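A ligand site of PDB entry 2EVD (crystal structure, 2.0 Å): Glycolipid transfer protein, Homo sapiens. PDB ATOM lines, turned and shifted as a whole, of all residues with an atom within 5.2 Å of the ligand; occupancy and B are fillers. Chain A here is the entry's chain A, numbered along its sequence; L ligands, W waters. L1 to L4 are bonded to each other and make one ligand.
An oxygen (O6) of LG2 L2 lies within hydrogen-bond range of the side-chain hydroxyl (OH) of Tyr 207 (2.6 Å).
The side-chain amide oxygen (OD1) of Asn 52 lies within hydrogen-bond range of an oxygen (O3) of LG2 L2 (2.5 Å).
A ring nitrogen (NE2) of His 140 is in hydrogen-bond range of an oxygen (O1) of LG4 L4 (2.9 Å).
O2 of LG2 L2 is in hydrogen-bond range of OD1 of Asp 48.
O of Asp 48 is in hydrogen-bond range of ND2 of Asn 52 (3.3 Å).
OH of Tyr 207 lies within hydrogen-bond range of NE1 of Trp 96 (2.8 Å).
Water W3 bridges O1 of LIG L1 (2.7 Å) and O of Gly 89 (2.8 Å).
CE1 of Phe 42 touches C11 of LG4 L4, at 3.8 Å.
CD1 of Ile 45 touches C10 of LG4 L4 (3.4 Å).
CD of Lys 55 touches O1 of LIG L1 (3.1 Å).
CD2 of Leu 92 touches O4 of LG2 L2, at 3.7 Å.
Trp 96 touches the ligand.
CA of Gly 100 touches C6 of LG4 L4, 3.9 Å away.
Phe 103 touches the ligand.
Leu 136 touches the ligand.
Phe 148 touches the ligand.
CB of Ala 151 touches C12 of LG4 L4, at 3.8 Å.
CG2 of Val 209 touches C1 of LG3 L3 (3.9 Å).
Within 4 Å of the ligand: Phe 42, Ile 45, Asp 48, Asn 52, Lys 55, Leu 92, Trp 96, Gly 100, Phe 103, Leu 136, His 140, Phe 148, Ala 151, Tyr 207 and Val 209.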
ATOM      1  N   PHE A  34      -9.700 -11.334   4.835  1.00  0.00           N
ATOM      2  CA  PHE A  34      -9.244 -12.683   4.509  1.00  0.00           C
ATOM      3  C   PHE A  34     -10.288 -13.526   3.779  1.00  0.00           C
ATOM      4  O   PHE A  34      -9.931 -14.442   3.033  1.00  0.00           O
ATOM      5  CB  PHE A  34      -8.688 -13.394   5.743  1.00  0.00           C
ATOM      6  CG  PHE A  34      -7.283 -12.985   6.084  1.00  0.00           C
ATOM      7  CD1 PHE A  34      -6.216 -13.476   5.348  1.00  0.00           C
ATOM      8  CD2 PHE A  34      -7.038 -12.088   7.115  1.00  0.00           C
ATOM      9  CE1 PHE A  34      -4.919 -13.093   5.656  1.00  0.00           C
ATOM     10  CE2 PHE A  34      -5.743 -11.697   7.416  1.00  0.00           C
ATOM     11  CZ  PHE A  34      -4.683 -12.212   6.703  1.00  0.00           C
ATOM     12  N   PHE A  42      -6.981 -19.552   3.569  1.00  0.00           N
ATOM     13  CA  PHE A  42      -6.916 -18.404   4.481  1.00  0.00           C
ATOM     14  C   PHE A  42      -7.767 -18.494   5.723  1.00  0.00           C
ATOM     15  O   PHE A  42      -7.513 -17.768   6.692  1.00  0.00           O
ATOM     16  CB  PHE A  42      -7.187 -17.106   3.700  1.00  0.00           C
ATOM     17  CG  PHE A  42      -6.212 -16.898   2.610  1.00  0.00           C
ATOM     18  CD1 PHE A  42      -4.907 -16.528   2.901  1.00  0.00           C
ATOM     19  CD2 PHE A  42      -6.540 -17.222   1.300  1.00  0.00           C
ATOM     20  CE1 PHE A  42      -3.943 -16.414   1.896  1.00  0.00           C
ATOM     21  CE2 PHE A  42      -5.591 -17.083   0.281  1.00  0.00           C
ATOM     22  CZ  PHE A  42      -4.299 -16.686   0.575  1.00  0.00           C
ATOM     23  N   PRO A  44      -7.974 -20.646   8.425  1.00  0.00           N
ATOM     24  CA  PRO A  44      -7.235 -20.745   9.696  1.00  0.00           C
ATOM     25  C   PRO A  44      -6.383 -19.515  10.052  1.00  0.00           C
ATOM     26  O   PRO A  44      -6.111 -19.254  11.212  1.00  0.00           O
ATOM     27  CB  PRO A  44      -6.318 -21.966   9.489  1.00  0.00           C
ATOM     28  CG  PRO A  44      -6.900 -22.702   8.330  1.00  0.00           C
ATOM     29  CD  PRO A  44      -7.532 -21.671   7.459  1.00  0.00           C
ATOM     30  N   ILE A  45      -5.940 -18.773   9.042  1.00  0.00           N
ATOM     31  CA  ILE A  45      -5.167 -17.567   9.251  1.00  0.00           C
ATOM     32  C   ILE A  45      -6.052 -16.476   9.879  1.00  0.00           C
ATOM     33  O   ILE A  45      -5.699 -15.865  10.914  1.00  0.00           O
ATOM     34  CB  ILE A  45      -4.593 -17.102   7.919  1.00  0.00           C
ATOM     35  CG1 ILE A  45      -3.541 -18.107   7.427  1.00  0.00           C
ATOM     36  CG2 ILE A  45      -3.980 -15.730   8.077  1.00  0.00           C
ATOM     37  CD1 ILE A  45      -2.960 -17.786   6.016  1.00  0.00           C
ATOM     38  N   ASP A  48      -6.773 -17.330  13.394  1.00  0.00           N
ATOM     39  CA  ASP A  48      -5.692 -17.079  14.357  1.00  0.00           C
ATOM     40  C   ASP A  48      -5.718 -15.610  14.771  1.00  0.00           C
ATOM     41  O   ASP A  48      -5.615 -15.293  15.963  1.00  0.00           O
ATOM     42  CB  ASP A  48      -4.313 -17.374  13.774  1.00  0.00           C
ATOM     43  CG  ASP A  48      -3.212 -17.149  14.792  1.00  0.00           C
ATOM     44  OD1 ASP A  48      -2.915 -18.064  15.577  1.00  0.00           O
ATOM     45  OD2 ASP A  48      -2.660 -16.037  14.819  1.00  0.00           O
ATOM     46  N   ILE A  49      -5.844 -14.711  13.803  1.00  0.00           N
ATOM     47  CA  ILE A  49      -5.766 -13.278  14.113  1.00  0.00           C
ATOM     48  C   ILE A  49      -7.027 -12.898  14.907  1.00  0.00           C
ATOM     49  O   ILE A  49      -6.937 -12.253  15.939  1.00  0.00           O
ATOM     50  CB  ILE A  49      -5.622 -12.417  12.844  1.00  0.00           C
ATOM     51  CG1 ILE A  49      -4.274 -12.720  12.130  1.00  0.00           C
ATOM     52  CG2 ILE A  49      -5.741 -10.934  13.188  1.00  0.00           C
ATOM     53  CD1 ILE A  49      -4.162 -12.290  10.659  1.00  0.00           C
ATOM     54  N   ASN A  52      -6.969 -14.016  18.506  1.00  0.00           N
ATOM     55  CA  ASN A  52      -6.118 -13.256  19.414  1.00  0.00           C
ATOM     56  C   ASN A  52      -6.785 -11.946  19.789  1.00  0.00           C
ATOM     57  O   ASN A  52      -6.749 -11.558  20.929  1.00  0.00           O
ATOM     58  CB  ASN A  52      -4.740 -13.049  18.791  1.00  0.00           C
ATOM     59  CG  ASN A  52      -3.846 -14.278  18.957  1.00  0.00           C
ATOM     60  OD1 ASN A  52      -3.854 -14.929  19.994  1.00  0.00           O
ATOM     61  ND2 ASN A  52      -3.077 -14.582  17.928  1.00  0.00           N
ATOM     62  N   LYS A  55      -9.326 -12.816  22.451  1.00  0.00           N
ATOM     63  CA  LYS A  55      -8.687 -13.087  23.728  1.00  0.00           C
ATOM     64  C   LYS A  55      -8.282 -11.806  24.447  1.00  0.00           C
ATOM     65  O   LYS A  55      -8.483 -11.686  25.661  1.00  0.00           O
ATOM     66  CB  LYS A  55      -7.457 -14.002  23.534  1.00  0.00           C
ATOM     67  CG  LYS A  55      -7.869 -15.436  23.121  1.00  0.00           C
ATOM     68  CD  LYS A  55      -6.728 -16.329  22.609  1.00  0.00           C
ATOM     69  CE  LYS A  55      -7.322 -17.714  22.117  1.00  0.00           C
ATOM     70  NZ  LYS A  55      -6.626 -18.264  20.886  1.00  0.00           N
ATOM     71  N   GLY A  89      -2.159 -15.138  29.167  1.00  0.00           N
ATOM     72  CA  GLY A  89      -3.170 -14.083  29.085  1.00  0.00           C
ATOM     73  C   GLY A  89      -3.210 -13.248  27.825  1.00  0.00           C
ATOM     74  O   GLY A  89      -2.885 -13.748  26.750  1.00  0.00           O
ATOM     75  N   LEU A  92       0.228 -12.749  25.944  1.00  0.00           N
ATOM     76  CA  LEU A  92       0.620 -13.753  24.974  1.00  0.00           C
ATOM     77  C   LEU A  92      -0.161 -13.656  23.655  1.00  0.00           C
ATOM     78  O   LEU A  92       0.413 -13.818  22.547  1.00  0.00           O
ATOM     79  CB  LEU A  92       0.531 -15.168  25.583  1.00  0.00           C
ATOM     80  CG  LEU A  92       0.881 -16.325  24.646  1.00  0.00           C
ATOM     81  CD1 LEU A  92       2.362 -16.202  24.108  1.00  0.00           C
ATOM     82  CD2 LEU A  92       0.707 -17.603  25.460  1.00  0.00           C
ATOM     83  N   ALA A  93      -1.469 -13.432  23.749  1.00  0.00           N
ATOM     84  CA  ALA A  93      -2.278 -13.200  22.553  1.00  0.00           C
ATOM     85  C   ALA A  93      -1.780 -11.977  21.729  1.00  0.00           C
ATOM     86  O   ALA A  93      -1.691 -12.048  20.518  1.00  0.00           O
ATOM     87  CB  ALA A  93      -3.762 -13.006  22.932  1.00  0.00           C
ATOM     88  N   TRP A  96       1.392 -12.632  19.690  1.00  0.00           N
ATOM     89  CA  TRP A  96       1.146 -13.255  18.394  1.00  0.00           C
ATOM     90  C   TRP A  96       0.347 -12.366  17.449  1.00  0.00           C
ATOM     91  O   TRP A  96       0.573 -12.386  16.211  1.00  0.00           O
ATOM     92  CB  TRP A  96       0.493 -14.634  18.587  1.00  0.00           C
ATOM     93  CG  TRP A  96       1.515 -15.685  19.043  1.00  0.00           C
ATOM     94  CD1 TRP A  96       1.756 -16.106  20.321  1.00  0.00           C
ATOM     95  CD2 TRP A  96       2.478 -16.356  18.215  1.00  0.00           C
ATOM     96  NE1 TRP A  96       2.780 -17.027  20.329  1.00  0.00           N
ATOM     97  CE2 TRP A  96       3.232 -17.199  19.046  1.00  0.00           C
ATOM     98  CE3 TRP A  96       2.762 -16.322  16.835  1.00  0.00           C
ATOM     99  CZ2 TRP A  96       4.243 -18.028  18.543  1.00  0.00           C
ATOM    100  CZ3 TRP A  96       3.743 -17.141  16.339  1.00  0.00           C
ATOM    101  CH2 TRP A  96       4.480 -17.998  17.191  1.00  0.00           C
ATOM    102  N   GLY A 100       1.125 -11.076  13.370  1.00  0.00           N
ATOM    103  CA  GLY A 100       0.184 -11.097  12.253  1.00  0.00           C
ATOM    104  C   GLY A 100      -0.006  -9.702  11.650  1.00  0.00           C
ATOM    105  O   GLY A 100      -0.128  -9.563  10.421  1.00  0.00           O
ATOM    106  N   PHE A 103       3.075  -8.791   9.746  1.00  0.00           N
ATOM    107  CA  PHE A 103       2.995  -9.462   8.460  1.00  0.00           C
ATOM    108  C   PHE A 103       2.183  -8.635   7.484  1.00  0.00           C
ATOM    109  O   PHE A 103       2.646  -8.379   6.347  1.00  0.00           O
ATOM    110  CB  PHE A 103       2.431 -10.892   8.523  1.00  0.00           C
ATOM    111  CG  PHE A 103       2.286 -11.512   7.164  1.00  0.00           C
ATOM    112  CD1 PHE A 103       3.285 -12.354   6.652  1.00  0.00           C
ATOM    113  CD2 PHE A 103       1.161 -11.211   6.362  1.00  0.00           C
ATOM    114  CE1 PHE A 103       3.141 -12.900   5.370  1.00  0.00           C
ATOM    115  CE2 PHE A 103       1.025 -11.730   5.075  1.00  0.00           C
ATOM    116  CZ  PHE A 103       2.006 -12.589   4.568  1.00  0.00           C
ATOM    117  N   LEU A 136       7.172 -13.508  10.685  1.00  0.00           N
ATOM    118  CA  LEU A 136       6.696 -14.776  11.214  1.00  0.00           C
ATOM    119  C   LEU A 136       7.694 -15.917  11.210  1.00  0.00           C
ATOM    120  O   LEU A 136       7.693 -16.685  12.153  1.00  0.00           O
ATOM    121  CB  LEU A 136       5.440 -15.208  10.453  1.00  0.00           C
ATOM    122  CG  LEU A 136       4.173 -14.417  10.768  1.00  0.00           C
ATOM    123  CD1 LEU A 136       3.141 -14.755   9.696  1.00  0.00           C
ATOM    124  CD2 LEU A 136       3.656 -14.798  12.123  1.00  0.00           C
ATOM    125  N   HIS A 140       8.397 -20.041  13.591  1.00  0.00           N
ATOM    126  CA  HIS A 140       7.849 -21.259  13.064  1.00  0.00           C
ATOM    127  C   HIS A 140       8.951 -22.303  12.901  1.00  0.00           C
ATOM    128  O   HIS A 140      10.001 -22.015  12.302  1.00  0.00           O
ATOM    129  CB  HIS A 140       7.252 -21.005  11.680  1.00  0.00           C
ATOM    130  CG  HIS A 140       6.014 -20.156  11.703  1.00  0.00           C
ATOM    131  ND1 HIS A 140       5.352 -19.772  10.552  1.00  0.00           N
ATOM    132  CD2 HIS A 140       5.332 -19.614  12.740  1.00  0.00           C
ATOM    133  CE1 HIS A 140       4.295 -19.034  10.885  1.00  0.00           C
ATOM    134  NE2 HIS A 140       4.271 -18.926  12.202  1.00  0.00           N
ATOM    135  N   VAL A 144       5.521 -25.884   9.682  1.00  0.00           N
ATOM    136  CA  VAL A 144       4.618 -24.737   9.464  1.00  0.00           C
ATOM    137  C   VAL A 144       5.199 -23.841   8.371  1.00  0.00           C
ATOM    138  O   VAL A 144       4.496 -23.303   7.517  1.00  0.00           O
ATOM    139  CB  VAL A 144       4.395 -23.987  10.808  1.00  0.00           C
ATOM    140  CG1 VAL A 144       3.686 -22.627  10.593  1.00  0.00           C
ATOM    141  CG2 VAL A 144       3.615 -24.872  11.789  1.00  0.00           C
ATOM    142  N   ILE A 147       4.148 -25.588   5.262  1.00  0.00           N
ATOM    143  CA  ILE A 147       2.736 -25.232   4.995  1.00  0.00           C
ATOM    144  C   ILE A 147       2.585 -23.786   4.444  1.00  0.00           C
ATOM    145  O   ILE A 147       1.834 -23.552   3.483  1.00  0.00           O
ATOM    146  CB  ILE A 147       1.861 -25.499   6.254  1.00  0.00           C
ATOM    147  CG1 ILE A 147       1.765 -27.020   6.516  1.00  0.00           C
ATOM    148  CG2 ILE A 147       0.489 -24.818   6.075  1.00  0.00           C
ATOM    149  CD1 ILE A 147       1.390 -27.437   7.946  1.00  0.00           C
ATOM    150  N   PHE A 148       3.281 -22.814   5.018  1.00  0.00           N
ATOM    151  CA  PHE A 148       3.280 -21.462   4.451  1.00  0.00           C
ATOM    152  C   PHE A 148       3.682 -21.460   2.964  1.00  0.00           C
ATOM    153  O   PHE A 148       2.969 -20.911   2.110  1.00  0.00           O
ATOM    154  CB  PHE A 148       4.189 -20.493   5.199  1.00  0.00           C
ATOM    155  CG  PHE A 148       4.394 -19.192   4.443  1.00  0.00           C
ATOM    156  CD1 PHE A 148       3.402 -18.211   4.441  1.00  0.00           C
ATOM    157  CD2 PHE A 148       5.520 -19.001   3.641  1.00  0.00           C
ATOM    158  CE1 PHE A 148       3.549 -17.042   3.688  1.00  0.00           C
ATOM    159  CE2 PHE A 148       5.683 -17.835   2.892  1.00  0.00           C
ATOM    160  CZ  PHE A 148       4.709 -16.856   2.912  1.00  0.00           C
ATOM    161  N   ALA A 151       0.732 -22.868   1.014  1.00  0.00           N
ATOM    162  CA  ALA A 151      -0.342 -21.850   1.125  1.00  0.00           C
ATOM    163  C   ALA A 151      -0.109 -20.669   0.203  1.00  0.00           C
ATOM    164  O   ALA A 151      -1.049 -20.122  -0.377  1.00  0.00           O
ATOM    165  CB  ALA A 151      -0.452 -21.348   2.572  1.00  0.00           C
ATOM    166  N   LEU A 152       1.152 -20.279   0.068  1.00  0.00           N
ATOM    167  CA  LEU A 152       1.535 -19.178  -0.797  1.00  0.00           C
ATOM    168  C   LEU A 152       0.958 -19.294  -2.203  1.00  0.00           C
ATOM    169  O   LEU A 152       0.649 -18.292  -2.818  1.00  0.00           O
ATOM    170  CB  LEU A 152       3.053 -19.046  -0.848  1.00  0.00           C
ATOM    171  CG  LEU A 152       3.674 -17.913  -1.675  1.00  0.00           C
ATOM    172  CD1 LEU A 152       3.285 -16.588  -1.041  1.00  0.00           C
ATOM    173  CD2 LEU A 152       5.204 -18.091  -1.727  1.00  0.00           C
ATOM    174  N   TYR A 207      10.091 -18.675  21.265  1.00  0.00           N
ATOM    175  CA  TYR A 207       9.777 -20.064  21.012  1.00  0.00           C
ATOM    176  C   TYR A 207       9.154 -20.223  19.622  1.00  0.00           C
ATOM    177  O   TYR A 207       8.465 -19.319  19.117  1.00  0.00           O
ATOM    178  CB  TYR A 207       8.914 -20.669  22.122  1.00  0.00           C
ATOM    179  CG  TYR A 207       7.460 -20.240  22.112  1.00  0.00           C
ATOM    180  CD1 TYR A 207       6.505 -20.949  21.399  1.00  0.00           C
ATOM    181  CD2 TYR A 207       7.038 -19.132  22.858  1.00  0.00           C
ATOM    182  CE1 TYR A 207       5.185 -20.557  21.405  1.00  0.00           C
ATOM    183  CE2 TYR A 207       5.699 -18.730  22.852  1.00  0.00           C
ATOM    184  CZ  TYR A 207       4.791 -19.435  22.111  1.00  0.00           C
ATOM    185  OH  TYR A 207       3.467 -19.057  22.119  1.00  0.00           O
ATOM    186  N   VAL A 209       6.831 -22.630  16.832  1.00  0.00           N
ATOM    187  CA  VAL A 209       5.676 -23.529  16.858  1.00  0.00           C
ATOM    188  C   VAL A 209       5.683 -24.518  15.699  1.00  0.00           C
ATOM    189  O   VAL A 209       6.182 -24.274  14.595  1.00  0.00           O
ATOM    190  CB  VAL A 209       4.329 -22.757  16.973  1.00  0.00           C
ATOM    191  CG1 VAL A 209       4.153 -22.144  18.381  1.00  0.00           C
ATOM    192  CG2 VAL A 209       4.161 -21.712  15.876  1.00  0.00           C
ATOM    193  OXT VAL A 209       5.216 -25.641  15.795  1.00  0.00           O
HETATM  194  C1  LIG L   1      -2.213 -18.969  23.588  1.00  0.00           C
HETATM  195  C2  LIG L   1      -3.718 -18.723  23.433  1.00  0.00           C
HETATM  196  C3  LIG L   1      -4.459 -19.322  24.655  1.00  0.00           C
HETATM  197  C4  LIG L   1      -4.010 -20.773  24.838  1.00  0.00           C
HETATM  198  C5  LIG L   1      -2.478 -20.814  24.929  1.00  0.00           C
HETATM  199  C6  LIG L   1      -1.880 -22.171  25.306  1.00  0.00           C
HETATM  200  O1  LIG L   1      -3.902 -17.316  23.361  1.00  0.00           O
HETATM  201  O2  LIG L   1      -5.857 -19.238  24.485  1.00  0.00           O
HETATM  202  O3  LIG L   1      -4.413 -21.533  23.723  1.00  0.00           O
HETATM  203  O4  LIG L   1      -1.940 -20.356  23.707  1.00  0.00           O
HETATM  204  O5  LIG L   1      -0.599 -21.904  25.856  1.00  0.00           O
HETATM  205  C1  LG2 L   2      -1.905 -18.240  18.851  1.00  0.00           C
HETATM  206  C2  LG2 L   2      -1.862 -17.768  20.301  1.00  0.00           C
HETATM  207  C3  LG2 L   2      -1.509 -18.912  21.244  1.00  0.00           C
HETATM  208  C4  LG2 L   2      -0.113 -19.448  20.895  1.00  0.00           C
HETATM  209  C5  LG2 L   2       0.374 -20.606  21.775  1.00  0.00           C
HETATM  210  C6  LG2 L   2      -0.874 -19.351  18.524  1.00  0.00           C
HETATM  211  O1  LG2 L   2      -0.212 -19.184  17.311  1.00  0.00           O
HETATM  212  O2  LG2 L   2      -1.938 -17.172  17.937  1.00  0.00           O
HETATM  213  O3  LG2 L   2      -3.136 -17.264  20.631  1.00  0.00           O
HETATM  214  O4  LG2 L   2      -1.484 -18.350  22.541  1.00  0.00           O
HETATM  215  O5  LG2 L   2      -0.005 -19.830  19.529  1.00  0.00           O
HETATM  216  O6  LG2 L   2       1.739 -20.837  21.488  1.00  0.00           O
HETATM  217  C1  LG3 L   3       0.879 -19.701  16.718  1.00  0.00           C
HETATM  218  C2  LG3 L   3       0.735 -19.563  15.198  1.00  0.00           C
HETATM  219  N1  LG3 L   3       0.393 -18.197  14.842  1.00  0.00           N
HETATM  220  C3  LG3 L   3      -0.290 -20.569  14.677  1.00  0.00           C
HETATM  221  O1  LG3 L   3       0.153 -21.888  15.046  1.00  0.00           O
HETATM  222  C4  LG3 L   3      -0.474 -20.507  13.166  1.00  0.00           C
HETATM  223  C5  LG3 L   3      -1.688 -20.430  12.594  1.00  0.00           C
HETATM  224  C6  LG3 L   3      -1.910 -20.772  11.107  1.00  0.00           C
HETATM  225  C7  LG3 L   3      -2.236 -22.251  10.839  1.00  0.00           C
HETATM  226  C8  LG3 L   3      -1.055 -23.157  10.448  1.00  0.00           C
HETATM  227  C9  LG3 L   3      -1.278 -24.655  10.660  1.00  0.00           C
HETATM  228  C10 LG3 L   3      -1.986 -25.372   9.521  1.00  0.00           C
HETATM  229  C11 LG3 L   3      -2.151 -26.875   9.723  1.00  0.00           C
HETATM  230  C12 LG3 L   3      -3.187 -27.416   8.723  1.00  0.00           C
HETATM  231  C13 LG3 L   3      -3.020 -28.894   8.367  1.00  0.00           C
HETATM  232  C14 LG3 L   3      -4.256 -29.383   7.613  1.00  0.00           C
HETATM  233  C15 LG3 L   3      -4.170 -30.804   7.063  1.00  0.00           C
HETATM  234  C16 LG3 L   3      -4.741 -30.886   5.645  1.00  0.00           C
HETATM  235  C17 LG3 L   3      -6.185 -31.396   5.511  1.00  0.00           C
HETATM  236  C18 LG3 L   3      -6.328 -32.819   6.027  1.00  0.00           C
HETATM  237  O1  LG4 L   4       1.906 -17.700  13.429  1.00  0.00           O
HETATM  238  C1  LG4 L   4       0.811 -17.184  14.216  1.00  0.00           C
HETATM  239  C2  LG4 L   4       0.244 -15.943  13.542  1.00  0.00           C
HETATM  240  C3  LG4 L   4      -0.243 -16.237  12.125  1.00  0.00           C
HETATM  241  C4  LG4 L   4      -0.518 -14.896  11.450  1.00  0.00           C
HETATM  242  C5  LG4 L   4      -0.477 -15.003   9.920  1.00  0.00           C
HETATM  243  C6  LG4 L   4      -0.473 -13.611   9.287  1.00  0.00           C
HETATM  244  C7  LG4 L   4      -0.930 -13.695   7.842  1.00  0.00           C
HETATM  245  C8  LG4 L   4      -0.292 -14.897   7.142  1.00  0.00           C
HETATM  246  C9  LG4 L   4      -0.762 -14.993   5.688  1.00  0.00           C
HETATM  247  C10 LG4 L   4      -0.107 -16.181   4.968  1.00  0.00           C
HETATM  248  C11 LG4 L   4      -0.508 -16.272   3.494  1.00  0.00           C
HETATM  249  C12 LG4 L   4      -0.092 -17.599   2.893  1.00  0.00           C
HETATM  250  O   HOH W   1      -7.348 -18.570  26.500  1.00  0.00           O
HETATM  251  O   HOH W   2      -0.198 -22.672  17.859  1.00  0.00           O
HETATM  252  O   HOH W   3      -3.251 -16.364  25.842  1.00  0.00           O
HETATM  253  O   HOH W   4      -1.743 -23.734  14.183  1.00  0.00           O
